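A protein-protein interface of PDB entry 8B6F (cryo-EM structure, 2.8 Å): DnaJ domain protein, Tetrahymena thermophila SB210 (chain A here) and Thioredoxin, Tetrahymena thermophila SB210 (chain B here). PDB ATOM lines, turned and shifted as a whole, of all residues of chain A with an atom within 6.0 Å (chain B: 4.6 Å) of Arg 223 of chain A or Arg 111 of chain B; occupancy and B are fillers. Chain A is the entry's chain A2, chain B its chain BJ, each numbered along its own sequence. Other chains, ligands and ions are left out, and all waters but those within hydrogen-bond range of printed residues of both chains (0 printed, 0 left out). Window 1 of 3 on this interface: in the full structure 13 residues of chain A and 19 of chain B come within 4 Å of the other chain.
The guanidinium group (NH1) of Arg 223 of chain A lies within hydrogen-bond range of the backbone carbonyl oxygen (O) of Ala 93 of chain B (2.7 Å). The guanidinium group of Arg 223 of chain A lies close to the guanidinium group of Arg 111 of chain B. NH1 of Arg 223 of chain A lies within salt-bridge range of OE2 of Glu 99 of chain B (3.5 Å). The guanidinium group of Arg 95 of chain B lies within hydrogen-bond range of the backbone carbonyl oxygen of Arg 222 of chain A, 2.5 Å away.
The side-chain carboxylate (OE1) of Glu 108 of chain B is in salt-bridge range of the guanidinium group (NH2) of Arg 111 of chain B, 3.0 Å away. O of Phe 92 of chain B sits at hydrogen-bond distance from NH1 of Arg 111 of chain B. The side-chain hydroxyl (OG1) of Thr 113 of chain B lies within hydrogen-bond range of the side-chain carboxylate (OE1) of Glu 99 of chain B (2.9 Å).
Among the printed residues, merely in contact across the chains: Glu 221 of chain A with Arg 95 of chain B (3.8 Å), Arg 222 of chain A with Tyr 150 of chain B (3.5 Å), Arg 223 of chain A with Arg 95 of chain B (3.2 Å), Arg 223 of chain A with Glu 108 of chain B (3.9 Å), Arg 223 of chain A with Tyr 150 of chain B (3.7 Å), Lys 224 of chain A with Ala 93 of chain B (3.2 Å), Lys 224 of chain A with Tyr 150 of chain B (3.5 Å) and Ser 225 of chain A with Tyr 150 of chain B (3.4 Å).
Arg 223 of chain A touches just these residues of chain B: Ala 93 (2.7 Å), Arg 95 (3.2 Å), Glu 99 (3.5 Å), Glu 108 (3.9 Å), Arg 111 (3.2 Å) and Tyr 150 (3.7 Å). Arg 111 of chain B touches one residue of chain A. Printed residues of chain A within 4 Å of Glu 108 of chain B: Arg 223. Of the printed residues of chain B, Glu 221 of chain A touches Arg 95 (3.8 Å). Of the printed residues of chain A, Tyr 150 of chain B touches Arg 222, Arg 223, Lys 224 and Ser 225. The nearest residue of chain B that does not touch Arg 223 of chain A is Val 94 of chain B (4.4 Å). The nearest printed residue of chain A that does not touch Arg 111 of chain B is Lys 224 of chain A (6.7 Å). The nearest printed residue of chain B that does not touch Lys 224 of chain A is Arg 95 of chain B (5.0 Å).
Printed residues of chain A that touch a printed residue of chain B: Glu 221, Arg 222, Arg 223, Lys 224 and Ser 225. Hydrophobic or aromatic side chains of chain B that line the printed part of chain A: Ala 93 and Tyr 150.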
ATOM      1  N   VAL A 219     -13.766 -18.248   6.523  1.00  0.00           N
ATOM      2  CA  VAL A 219     -15.107 -18.788   6.330  1.00  0.00           C
ATOM      3  C   VAL A 219     -15.485 -18.774   4.855  1.00  0.00           C
ATOM      4  O   VAL A 219     -16.157 -19.689   4.366  1.00  0.00           O
ATOM      5  CB  VAL A 219     -16.122 -18.002   7.181  1.00  0.00           C
ATOM      6  CG1 VAL A 219     -17.523 -18.570   7.008  1.00  0.00           C
ATOM      7  CG2 VAL A 219     -15.715 -18.023   8.646  1.00  0.00           C
ATOM      8  N   GLU A 221     -13.595 -19.156   2.178  1.00  0.00           N
ATOM      9  CA  GLU A 221     -12.913 -20.202   1.430  1.00  0.00           C
ATOM     10  C   GLU A 221     -13.082 -21.583   2.047  1.00  0.00           C
ATOM     11  O   GLU A 221     -12.538 -22.553   1.510  1.00  0.00           O
ATOM     12  CB  GLU A 221     -11.421 -19.873   1.310  1.00  0.00           C
ATOM     13  CG  GLU A 221     -10.682 -19.849   2.635  1.00  0.00           C
ATOM     14  CD  GLU A 221      -9.234 -19.434   2.478  1.00  0.00           C
ATOM     15  OE1 GLU A 221      -8.874 -18.935   1.392  1.00  0.00           O
ATOM     16  OE2 GLU A 221      -8.454 -19.613   3.438  1.00  0.00           O
ATOM     17  N   ARG A 222     -13.811 -21.699   3.152  1.00  0.00           N
ATOM     18  CA  ARG A 222     -14.037 -23.000   3.765  1.00  0.00           C
ATOM     19  C   ARG A 222     -14.902 -23.860   2.853  1.00  0.00           C
ATOM     20  O   ARG A 222     -15.927 -23.402   2.339  1.00  0.00           O
ATOM     21  CB  ARG A 222     -14.701 -22.831   5.128  1.00  0.00           C
ATOM     22  CG  ARG A 222     -14.903 -24.130   5.882  1.00  0.00           C
ATOM     23  CD  ARG A 222     -15.553 -23.885   7.231  1.00  0.00           C
ATOM     24  NE  ARG A 222     -15.796 -25.131   7.945  1.00  0.00           N
ATOM     25  CZ  ARG A 222     -16.350 -25.210   9.147  1.00  0.00           C
ATOM     26  NH1 ARG A 222     -16.731 -24.129   9.805  1.00  0.00           N
ATOM     27  NH2 ARG A 222     -16.524 -26.405   9.704  1.00  0.00           N
ATOM     28  N   ARG A 223     -14.489 -25.110   2.656  1.00  0.00           N
ATOM     29  CA  ARG A 223     -15.193 -26.052   1.792  1.00  0.00           C
ATOM     30  C   ARG A 223     -16.048 -26.964   2.664  1.00  0.00           C
ATOM     31  O   ARG A 223     -15.519 -27.777   3.426  1.00  0.00           O
ATOM     32  CB  ARG A 223     -14.204 -26.859   0.956  1.00  0.00           C
ATOM     33  CG  ARG A 223     -13.411 -26.026  -0.035  1.00  0.00           C
ATOM     34  CD  ARG A 223     -14.270 -25.589  -1.209  1.00  0.00           C
ATOM     35  NE  ARG A 223     -13.523 -24.764  -2.150  1.00  0.00           N
ATOM     36  CZ  ARG A 223     -13.974 -24.389  -3.339  1.00  0.00           C
ATOM     37  NH1 ARG A 223     -15.164 -24.764  -3.776  1.00  0.00           N
ATOM     38  NH2 ARG A 223     -13.211 -23.620  -4.109  1.00  0.00           N
ATOM     39  N   LYS A 224     -17.365 -26.835   2.538  1.00  0.00           N
ATOM     40  CA  LYS A 224     -18.317 -27.583   3.345  1.00  0.00           C
ATOM     41  C   LYS A 224     -18.980 -28.649   2.484  1.00  0.00           C
ATOM     42  O   LYS A 224     -19.466 -28.353   1.389  1.00  0.00           O
ATOM     43  CB  LYS A 224     -19.370 -26.649   3.944  1.00  0.00           C
ATOM     44  CG  LYS A 224     -18.775 -25.452   4.679  1.00  0.00           C
ATOM     45  CD  LYS A 224     -19.842 -24.632   5.389  1.00  0.00           C
ATOM     46  CE  LYS A 224     -20.757 -23.914   4.410  1.00  0.00           C
ATOM     47  NZ  LYS A 224     -20.013 -22.964   3.535  1.00  0.00           N
ATOM     48  N   SER A 225     -19.008 -29.879   2.985  1.00  0.00           N
ATOM     49  CA  SER A 225     -19.549 -31.018   2.256  1.00  0.00           C
ATOM     50  C   SER A 225     -20.956 -31.325   2.749  1.00  0.00           C
ATOM     51  O   SER A 225     -21.194 -31.391   3.959  1.00  0.00           O
ATOM     52  CB  SER A 225     -18.652 -32.245   2.423  1.00  0.00           C
ATOM     53  OG  SER A 225     -18.465 -32.556   3.792  1.00  0.00           O
ATOM     54  N   PHE B  92     -18.781 -32.535  -2.639  1.00  0.00           N
ATOM     55  CA  PHE B  92     -17.408 -32.086  -2.822  1.00  0.00           C
ATOM     56  C   PHE B  92     -17.268 -30.572  -2.759  1.00  0.00           C
ATOM     57  O   PHE B  92     -16.179 -30.052  -3.017  1.00  0.00           O
ATOM     58  CB  PHE B  92     -16.857 -32.606  -4.152  1.00  0.00           C
ATOM     59  CG  PHE B  92     -16.655 -34.091  -4.180  1.00  0.00           C
ATOM     60  CD1 PHE B  92     -15.547 -34.659  -3.578  1.00  0.00           C
ATOM     61  CD2 PHE B  92     -17.571 -34.918  -4.803  1.00  0.00           C
ATOM     62  CE1 PHE B  92     -15.355 -36.025  -3.596  1.00  0.00           C
ATOM     63  CE2 PHE B  92     -17.385 -36.288  -4.825  1.00  0.00           C
ATOM     64  CZ  PHE B  92     -16.275 -36.841  -4.222  1.00  0.00           C
ATOM     65  N   ALA B  93     -18.340 -29.854  -2.427  1.00  0.00           N
ATOM     66  CA  ALA B  93     -18.269 -28.412  -2.208  1.00  0.00           C
ATOM     67  C   ALA B  93     -17.780 -27.690  -3.458  1.00  0.00           C
ATOM     68  O   ALA B  93     -17.025 -26.720  -3.383  1.00  0.00           O
ATOM     69  CB  ALA B  93     -17.377 -28.084  -1.011  1.00  0.00           C
ATOM     70  N   VAL B  94     -18.214 -28.168  -4.617  1.00  0.00           N
ATOM     71  CA  VAL B  94     -17.867 -27.532  -5.882  1.00  0.00           C
ATOM     72  C   VAL B  94     -18.693 -26.263  -6.037  1.00  0.00           C
ATOM     73  O   VAL B  94     -19.924 -26.290  -5.933  1.00  0.00           O
ATOM     74  CB  VAL B  94     -18.105 -28.496  -7.055  1.00  0.00           C
ATOM     75  CG1 VAL B  94     -17.667 -27.862  -8.369  1.00  0.00           C
ATOM     76  CG2 VAL B  94     -17.381 -29.809  -6.819  1.00  0.00           C
ATOM     77  N   ARG B  95     -18.013 -25.143  -6.283  1.00  0.00           N
ATOM     78  CA  ARG B  95     -18.659 -23.847  -6.446  1.00  0.00           C
ATOM     79  C   ARG B  95     -18.709 -23.404  -7.902  1.00  0.00           C
ATOM     80  O   ARG B  95     -19.775 -23.042  -8.405  1.00  0.00           O
ATOM     81  CB  ARG B  95     -17.929 -22.795  -5.605  1.00  0.00           C
ATOM     82  CG  ARG B  95     -17.955 -23.084  -4.114  1.00  0.00           C
ATOM     83  CD  ARG B  95     -17.041 -22.146  -3.348  1.00  0.00           C
ATOM     84  NE  ARG B  95     -17.048 -22.430  -1.919  1.00  0.00           N
ATOM     85  CZ  ARG B  95     -16.294 -21.803  -1.027  1.00  0.00           C
ATOM     86  NH1 ARG B  95     -15.452 -20.847  -1.385  1.00  0.00           N
ATOM     87  NH2 ARG B  95     -16.386 -22.142   0.255  1.00  0.00           N
ATOM     88  N   GLU B  99     -13.787 -28.039 -12.126  1.00  0.00           N
ATOM     89  CA  GLU B  99     -13.138 -28.060 -10.826  1.00  0.00           C
ATOM     90  C   GLU B  99     -12.177 -29.236 -10.771  1.00  0.00           C
ATOM     91  O   GLU B  99     -12.544 -30.355 -11.141  1.00  0.00           O
ATOM     92  CB  GLU B  99     -14.176 -28.179  -9.708  1.00  0.00           C
ATOM     93  CG  GLU B  99     -13.712 -27.692  -8.349  1.00  0.00           C
ATOM     94  CD  GLU B  99     -13.924 -26.203  -8.169  1.00  0.00           C
ATOM     95  OE1 GLU B  99     -13.753 -25.452  -9.150  1.00  0.00           O
ATOM     96  OE2 GLU B  99     -14.279 -25.782  -7.048  1.00  0.00           O
ATOM     97  N   PHE B 100     -10.954 -28.986 -10.317  1.00  0.00           N
ATOM     98  CA  PHE B 100      -9.966 -30.032 -10.102  1.00  0.00           C
ATOM     99  C   PHE B 100      -9.635 -30.072  -8.619  1.00  0.00           C
ATOM    100  O   PHE B 100      -9.353 -29.032  -8.017  1.00  0.00           O
ATOM    101  CB  PHE B 100      -8.704 -29.789 -10.932  1.00  0.00           C
ATOM    102  CG  PHE B 100      -8.953 -29.735 -12.409  1.00  0.00           C
ATOM    103  CD1 PHE B 100      -8.910 -30.888 -13.172  1.00  0.00           C
ATOM    104  CD2 PHE B 100      -9.228 -28.532 -13.036  1.00  0.00           C
ATOM    105  CE1 PHE B 100      -9.137 -30.842 -14.534  1.00  0.00           C
ATOM    106  CE2 PHE B 100      -9.454 -28.479 -14.397  1.00  0.00           C
ATOM    107  CZ  PHE B 100      -9.410 -29.636 -15.147  1.00  0.00           C
ATOM    108  N   LEU B 101      -9.669 -31.265  -8.036  1.00  0.00           N
ATOM    109  CA  LEU B 101      -9.462 -31.438  -6.607  1.00  0.00           C
ATOM    110  C   LEU B 101      -8.414 -32.514  -6.384  1.00  0.00           C
ATOM    111  O   LEU B 101      -8.557 -33.634  -6.883  1.00  0.00           O
ATOM    112  CB  LEU B 101     -10.777 -31.808  -5.913  1.00  0.00           C
ATOM    113  CG  LEU B 101     -10.726 -32.118  -4.418  1.00  0.00           C
ATOM    114  CD1 LEU B 101     -10.207 -30.929  -3.631  1.00  0.00           C
ATOM    115  CD2 LEU B 101     -12.103 -32.523  -3.930  1.00  0.00           C
ATOM    116  N   GLU B 108      -8.287 -33.178   1.244  1.00  0.00           N
ATOM    117  CA  GLU B 108      -8.075 -32.119   0.267  1.00  0.00           C
ATOM    118  C   GLU B 108      -6.713 -31.471   0.460  1.00  0.00           C
ATOM    119  O   GLU B 108      -6.403 -30.962   1.542  1.00  0.00           O
ATOM    120  CB  GLU B 108      -9.180 -31.071   0.378  1.00  0.00           C
ATOM    121  CG  GLU B 108      -8.935 -29.834  -0.478  1.00  0.00           C
ATOM    122  CD  GLU B 108     -10.137 -28.916  -0.545  1.00  0.00           C
ATOM    123  OE1 GLU B 108     -11.220 -29.312  -0.066  1.00  0.00           O
ATOM    124  OE2 GLU B 108      -9.999 -27.793  -1.076  1.00  0.00           O
ATOM    125  N   THR B 110      -5.275 -29.479  -2.557  1.00  0.00           N
ATOM    126  CA  THR B 110      -5.365 -28.276  -3.367  1.00  0.00           C
ATOM    127  C   THR B 110      -6.583 -28.393  -4.269  1.00  0.00           C
ATOM    128  O   THR B 110      -7.109 -29.485  -4.496  1.00  0.00           O
ATOM    129  CB  THR B 110      -4.091 -28.064  -4.197  1.00  0.00           C
ATOM    130  OG1 THR B 110      -2.942 -28.198  -3.354  1.00  0.00           O
ATOM    131  CG2 THR B 110      -4.067 -26.680  -4.835  1.00  0.00           C
ATOM    132  N   ARG B 111      -7.030 -27.249  -4.775  1.00  0.00           N
ATOM    133  CA  ARG B 111      -8.182 -27.185  -5.658  1.00  0.00           C
ATOM    134  C   ARG B 111      -7.942 -26.102  -6.696  1.00  0.00           C
ATOM    135  O   ARG B 111      -7.428 -25.027  -6.376  1.00  0.00           O
ATOM    136  CB  ARG B 111      -9.470 -26.896  -4.878  1.00  0.00           C
ATOM    137  CG  ARG B 111     -10.737 -27.182  -5.660  1.00  0.00           C
ATOM    138  CD  ARG B 111     -11.955 -26.645  -4.938  1.00  0.00           C
ATOM    139  NE  ARG B 111     -12.185 -27.306  -3.659  1.00  0.00           N
ATOM    140  CZ  ARG B 111     -13.023 -28.317  -3.471  1.00  0.00           C
ATOM    141  NH1 ARG B 111     -13.727 -28.829  -4.467  1.00  0.00           N
ATOM    142  NH2 ARG B 111     -13.163 -28.825  -2.250  1.00  0.00           N
ATOM    143  N   GLN B 112      -8.312 -26.395  -7.936  1.00  0.00           N
ATOM    144  CA  GLN B 112      -8.165 -25.472  -9.049  1.00  0.00           C
ATOM    145  C   GLN B 112      -9.516 -25.245  -9.706  1.00  0.00           C
ATOM    146  O   GLN B 112     -10.286 -26.188  -9.908  1.00  0.00           O
ATOM    147  CB  GLN B 112      -7.170 -25.997 -10.086  1.00  0.00           C
ATOM    148  CG  GLN B 112      -7.156 -25.195 -11.382  1.00  0.00           C
ATOM    149  CD  GLN B 112      -6.018 -25.583 -12.296  1.00  0.00           C
ATOM    150  OE1 GLN B 112      -5.003 -26.111 -11.851  1.00  0.00           O
ATOM    151  NE2 GLN B 112      -6.182 -25.321 -13.587  1.00  0.00           N
ATOM    152  N   THR B 113      -9.794 -23.991 -10.038  1.00  0.00           N
ATOM    153  CA  THR B 113     -11.003 -23.615 -10.751  1.00  0.00           C
ATOM    154  C   THR B 113     -10.598 -23.080 -12.112  1.00  0.00           C
ATOM    155  O   THR B 113      -9.704 -22.234 -12.211  1.00  0.00           O
ATOM    156  CB  THR B 113     -11.794 -22.554  -9.980  1.00  0.00           C
ATOM    157  OG1 THR B 113     -12.131 -23.048  -8.677  1.00  0.00           O
ATOM    158  CG2 THR B 113     -13.071 -22.181 -10.719  1.00  0.00           C
ATOM    159  N   ARG B 123       0.207 -27.926 -10.075  1.00  0.00           N
ATOM    160  CA  ARG B 123      -0.376 -28.327  -8.799  1.00  0.00           C
ATOM    161  C   ARG B 123      -0.119 -29.801  -8.521  1.00  0.00           C
ATOM    162  O   ARG B 123       0.205 -30.179  -7.390  1.00  0.00           O
ATOM    163  CB  ARG B 123      -1.875 -28.033  -8.791  1.00  0.00           C
ATOM    164  CG  ARG B 123      -2.204 -26.553  -8.809  1.00  0.00           C
ATOM    165  CD  ARG B 123      -3.703 -26.317  -8.822  1.00  0.00           C
ATOM    166  NE  ARG B 123      -4.023 -24.925  -9.114  1.00  0.00           N
ATOM    167  CZ  ARG B 123      -4.049 -23.951  -8.215  1.00  0.00           C
ATOM    168  NH1 ARG B 123      -3.768 -24.176  -6.942  1.00  0.00           N
ATOM    169  NH2 ARG B 123      -4.363 -22.718  -8.602  1.00  0.00           N
ATOM    170  N   PHE B 146     -13.825 -37.854   2.125  1.00  0.00           N
ATOM    171  CA  PHE B 146     -13.621 -36.422   1.945  1.00  0.00           C
ATOM    172  C   PHE B 146     -14.250 -35.620   3.078  1.00  0.00           C
ATOM    173  O   PHE B 146     -13.705 -34.593   3.497  1.00  0.00           O
ATOM    174  CB  PHE B 146     -14.190 -35.978   0.599  1.00  0.00           C
ATOM    175  CG  PHE B 146     -14.048 -34.508   0.341  1.00  0.00           C
ATOM    176  CD1 PHE B 146     -12.851 -33.986  -0.113  1.00  0.00           C
ATOM    177  CD2 PHE B 146     -15.114 -33.650   0.546  1.00  0.00           C
ATOM    178  CE1 PHE B 146     -12.716 -32.636  -0.352  1.00  0.00           C
ATOM    179  CE2 PHE B 146     -14.987 -32.297   0.308  1.00  0.00           C
ATOM    180  CZ  PHE B 146     -13.785 -31.789  -0.141  1.00  0.00           C
ATOM    181  N   TYR B 150     -14.003 -32.225   7.475  1.00  0.00           N
ATOM    182  CA  TYR B 150     -14.995 -31.174   7.653  1.00  0.00           C
ATOM    183  C   TYR B 150     -15.918 -31.477   8.827  1.00  0.00           C
ATOM    184  O   TYR B 150     -16.247 -30.582   9.613  1.00  0.00           O
ATOM    185  CB  TYR B 150     -15.812 -30.986   6.376  1.00  0.00           C
ATOM    186  CG  TYR B 150     -17.031 -30.123   6.590  1.00  0.00           C
ATOM    187  CD1 TYR B 150     -16.912 -28.751   6.762  1.00  0.00           C
ATOM    188  CD2 TYR B 150     -18.301 -30.680   6.634  1.00  0.00           C
ATOM    189  CE1 TYR B 150     -18.021 -27.959   6.967  1.00  0.00           C
ATOM    190  CE2 TYR B 150     -19.418 -29.896   6.839  1.00  0.00           C
ATOM    191  CZ  TYR B 150     -19.271 -28.536   7.004  1.00  0.00           C
ATOM    192  OH  TYR B 150     -20.382 -27.751   7.206  1.00  0.00           O
